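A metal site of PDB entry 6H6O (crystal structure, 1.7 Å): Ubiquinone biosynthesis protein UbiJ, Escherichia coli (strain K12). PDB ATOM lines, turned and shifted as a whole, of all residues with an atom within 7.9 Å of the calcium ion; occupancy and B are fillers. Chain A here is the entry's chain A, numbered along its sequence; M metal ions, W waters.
Of the 13 residues printed, 3 come within 4 Å of the calcium ion.
The nearest printed residue that does not touch the calcium ion is Asp 94 (4.7 Å).
The calcium ion is bound by O of Arg 93, water W1, water W2, OD1 of Asp 124 and OE1 of Glu 127.
The calcium ion has five donor atoms within binding distance.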
ATOM      1  N   LYS A  91      18.438  -6.728  -8.702  1.00  0.00           N
ATOM      2  CA  LYS A  91      17.995  -6.800 -10.100  1.00  0.00           C
ATOM      3  C   LYS A  91      16.480  -6.648 -10.249  1.00  0.00           C
ATOM      4  O   LYS A  91      16.019  -6.395 -11.362  1.00  0.00           O
ATOM      5  CB  LYS A  91      18.412  -8.118 -10.761  1.00  0.00           C
ATOM      6  CG  LYS A  91      19.916  -8.331 -10.862  1.00  0.00           C
ATOM      7  CD  LYS A  91      20.248  -9.700 -11.373  1.00  0.00           C
ATOM      8  CE  LYS A  91      21.732  -9.929 -11.379  1.00  0.00           C
ATOM      9  NZ  LYS A  91      22.072 -11.237 -11.976  1.00  0.00           N
ATOM     10  N   LEU A  92      15.722  -6.892  -9.175  1.00  0.00           N
ATOM     11  CA  LEU A  92      14.263  -6.817  -9.207  1.00  0.00           C
ATOM     12  C   LEU A  92      13.739  -5.353  -9.234  1.00  0.00           C
ATOM     13  O   LEU A  92      12.955  -4.945  -8.381  1.00  0.00           O
ATOM     14  CB  LEU A  92      13.653  -7.650  -8.046  1.00  0.00           C
ATOM     15  CG  LEU A  92      13.890  -9.169  -8.094  1.00  0.00           C
ATOM     16  CD1 LEU A  92      13.503  -9.837  -6.772  1.00  0.00           C
ATOM     17  CD2 LEU A  92      13.096  -9.815  -9.199  1.00  0.00           C
ATOM     18  N   ARG A  93      14.179  -4.587 -10.262  1.00  0.00           N
ATOM     19  CA  ARG A  93      13.826  -3.180 -10.463  1.00  0.00           C
ATOM     20  C   ARG A  93      12.379  -2.965 -10.902  1.00  0.00           C
ATOM     21  O   ARG A  93      11.755  -1.990 -10.496  1.00  0.00           O
ATOM     22  CB  ARG A  93      14.784  -2.508 -11.450  1.00  0.00           C
ATOM     23  CG  ARG A  93      16.235  -2.454 -10.961  1.00  0.00           C
ATOM     24  CD  ARG A  93      17.186  -2.015 -12.055  1.00  0.00           C
ATOM     25  NE  ARG A  93      18.575  -1.995 -11.585  1.00  0.00           N
ATOM     26  CZ  ARG A  93      19.422  -3.022 -11.678  1.00  0.00           C
ATOM     27  NH1 ARG A  93      20.661  -2.914 -11.223  1.00  0.00           N
ATOM     28  NH2 ARG A  93      19.024  -4.167 -12.226  1.00  0.00           N
ATOM     29  N   ASP A  94      11.844  -3.873 -11.749  1.00  0.00           N
ATOM     30  CA  ASP A  94      10.477  -3.805 -12.285  1.00  0.00           C
ATOM     31  C   ASP A  94      10.030  -5.171 -12.831  1.00  0.00           C
ATOM     32  O   ASP A  94      10.820  -6.116 -12.833  1.00  0.00           O
ATOM     33  CB  ASP A  94      10.366  -2.710 -13.382  1.00  0.00           C
ATOM     34  CG  ASP A  94      11.493  -2.699 -14.410  1.00  0.00           C
ATOM     35  OD1 ASP A  94      11.909  -3.803 -14.850  1.00  0.00           O
ATOM     36  OD2 ASP A  94      11.909  -1.599 -14.814  1.00  0.00           O
ATOM     37  N   ARG A  95       8.760  -5.271 -13.294  1.00  0.00           N
ATOM     38  CA  ARG A  95       8.175  -6.486 -13.877  1.00  0.00           C
ATOM     39  C   ARG A  95       8.977  -7.009 -15.089  1.00  0.00           C
ATOM     40  O   ARG A  95       9.047  -8.220 -15.265  1.00  0.00           O
ATOM     41  CB  ARG A  95       6.666  -6.280 -14.199  1.00  0.00           C
ATOM     42  CG  ARG A  95       5.950  -7.421 -14.965  1.00  0.00           C
ATOM     43  CD  ARG A  95       5.989  -8.794 -14.287  1.00  0.00           C
ATOM     44  NE  ARG A  95       5.807  -9.877 -15.250  1.00  0.00           N
ATOM     45  CZ  ARG A  95       6.254 -11.122 -15.096  1.00  0.00           C
ATOM     46  NH1 ARG A  95       6.945 -11.449 -14.016  1.00  0.00           N
ATOM     47  NH2 ARG A  95       6.028 -12.039 -16.024  1.00  0.00           N
ATOM     48  N   VAL A 120       7.018  -6.921  -6.508  1.00  0.00           N
ATOM     49  CA  VAL A 120       7.997  -6.188  -7.325  1.00  0.00           C
ATOM     50  C   VAL A 120       7.386  -4.822  -7.778  1.00  0.00           C
ATOM     51  O   VAL A 120       8.047  -3.783  -7.665  1.00  0.00           O
ATOM     52  CB  VAL A 120       8.546  -7.080  -8.484  1.00  0.00           C
ATOM     53  CG1 VAL A 120       9.400  -6.277  -9.479  1.00  0.00           C
ATOM     54  CG2 VAL A 120       9.319  -8.280  -7.917  1.00  0.00           C
ATOM     55  N   ALA A 121       6.111  -4.833  -8.224  1.00  0.00           N
ATOM     56  CA  ALA A 121       5.374  -3.630  -8.610  1.00  0.00           C
ATOM     57  C   ALA A 121       5.288  -2.659  -7.413  1.00  0.00           C
ATOM     58  O   ALA A 121       5.513  -1.471  -7.581  1.00  0.00           O
ATOM     59  CB  ALA A 121       3.982  -3.988  -9.097  1.00  0.00           C
ATOM     60  N   ALA A 123       7.387  -2.578  -4.693  1.00  0.00           N
ATOM     61  CA  ALA A 123       8.740  -2.066  -4.425  1.00  0.00           C
ATOM     62  C   ALA A 123       9.117  -0.955  -5.438  1.00  0.00           C
ATOM     63  O   ALA A 123       9.719   0.062  -5.051  1.00  0.00           O
ATOM     64  CB  ALA A 123       9.755  -3.191  -4.463  1.00  0.00           C
ATOM     65  N   ASP A 124       8.723  -1.148  -6.726  1.00  0.00           N
ATOM     66  CA  ASP A 124       8.966  -0.168  -7.793  1.00  0.00           C
ATOM     67  C   ASP A 124       8.241   1.160  -7.460  1.00  0.00           C
ATOM     68  O   ASP A 124       8.851   2.220  -7.510  1.00  0.00           O
ATOM     69  CB  ASP A 124       8.497  -0.728  -9.151  1.00  0.00           C
ATOM     70  CG  ASP A 124       9.023   0.036 -10.365  1.00  0.00           C
ATOM     71  OD1 ASP A 124       9.907   0.893 -10.201  1.00  0.00           O
ATOM     72  OD2 ASP A 124       8.545  -0.245 -11.498  1.00  0.00           O
ATOM     73  N   LEU A 125       6.970   1.064  -7.020  1.00  0.00           N
ATOM     74  CA  LEU A 125       6.205   2.252  -6.670  1.00  0.00           C
ATOM     75  C   LEU A 125       6.707   2.892  -5.380  1.00  0.00           C
ATOM     76  O   LEU A 125       6.620   4.112  -5.244  1.00  0.00           O
ATOM     77  CB  LEU A 125       4.713   1.923  -6.594  1.00  0.00           C
ATOM     78  CG  LEU A 125       4.049   1.639  -7.968  1.00  0.00           C
ATOM     79  CD1 LEU A 125       2.669   1.060  -7.811  1.00  0.00           C
ATOM     80  CD2 LEU A 125       3.972   2.911  -8.844  1.00  0.00           C
ATOM     81  N   ALA A 126       7.265   2.086  -4.450  1.00  0.00           N
ATOM     82  CA  ALA A 126       7.821   2.589  -3.202  1.00  0.00           C
ATOM     83  C   ALA A 126       9.074   3.442  -3.423  1.00  0.00           C
ATOM     84  O   ALA A 126       9.376   4.357  -2.637  1.00  0.00           O
ATOM     85  CB  ALA A 126       8.096   1.447  -2.213  1.00  0.00           C
ATOM     86  N   GLU A 127       9.794   3.155  -4.507  1.00  0.00           N
ATOM     87  CA  GLU A 127      10.969   3.923  -4.919  1.00  0.00           C
ATOM     88  C   GLU A 127      10.494   5.213  -5.619  1.00  0.00           C
ATOM     89  O   GLU A 127      11.087   6.281  -5.422  1.00  0.00           O
ATOM     90  CB  GLU A 127      11.822   3.098  -5.861  1.00  0.00           C
ATOM     91  CG  GLU A 127      13.248   3.587  -6.000  1.00  0.00           C
ATOM     92  CD  GLU A 127      14.067   2.905  -7.090  1.00  0.00           C
ATOM     93  OE1 GLU A 127      13.473   2.218  -7.950  1.00  0.00           O
ATOM     94  OE2 GLU A 127      15.302   3.110  -7.105  1.00  0.00           O
ATOM     95  N   PHE A 128       9.411   5.114  -6.437  1.00  0.00           N
ATOM     96  CA  PHE A 128       8.830   6.256  -7.152  1.00  0.00           C
ATOM     97  C   PHE A 128       8.321   7.313  -6.161  1.00  0.00           C
ATOM     98  O   PHE A 128       8.512   8.510  -6.352  1.00  0.00           O
ATOM     99  CB  PHE A 128       7.692   5.797  -8.093  1.00  0.00           C
ATOM    100  CG  PHE A 128       6.598   6.828  -8.353  1.00  0.00           C
ATOM    101  CD1 PHE A 128       6.825   7.896  -9.221  1.00  0.00           C
ATOM    102  CD2 PHE A 128       5.374   6.742  -7.705  1.00  0.00           C
ATOM    103  CE1 PHE A 128       5.836   8.861  -9.428  1.00  0.00           C
ATOM    104  CE2 PHE A 128       4.385   7.720  -7.905  1.00  0.00           C
ATOM    105  CZ  PHE A 128       4.625   8.767  -8.768  1.00  0.00           C
HETATM  106 CA    CA M   1      12.488   0.328  -9.848  1.00  0.00          CA
HETATM  107  O   HOH W   1      12.081   2.488 -11.166  1.00  0.00           O
HETATM  108  O   HOH W   2      12.358  -1.198  -7.755  1.00  0.00           O
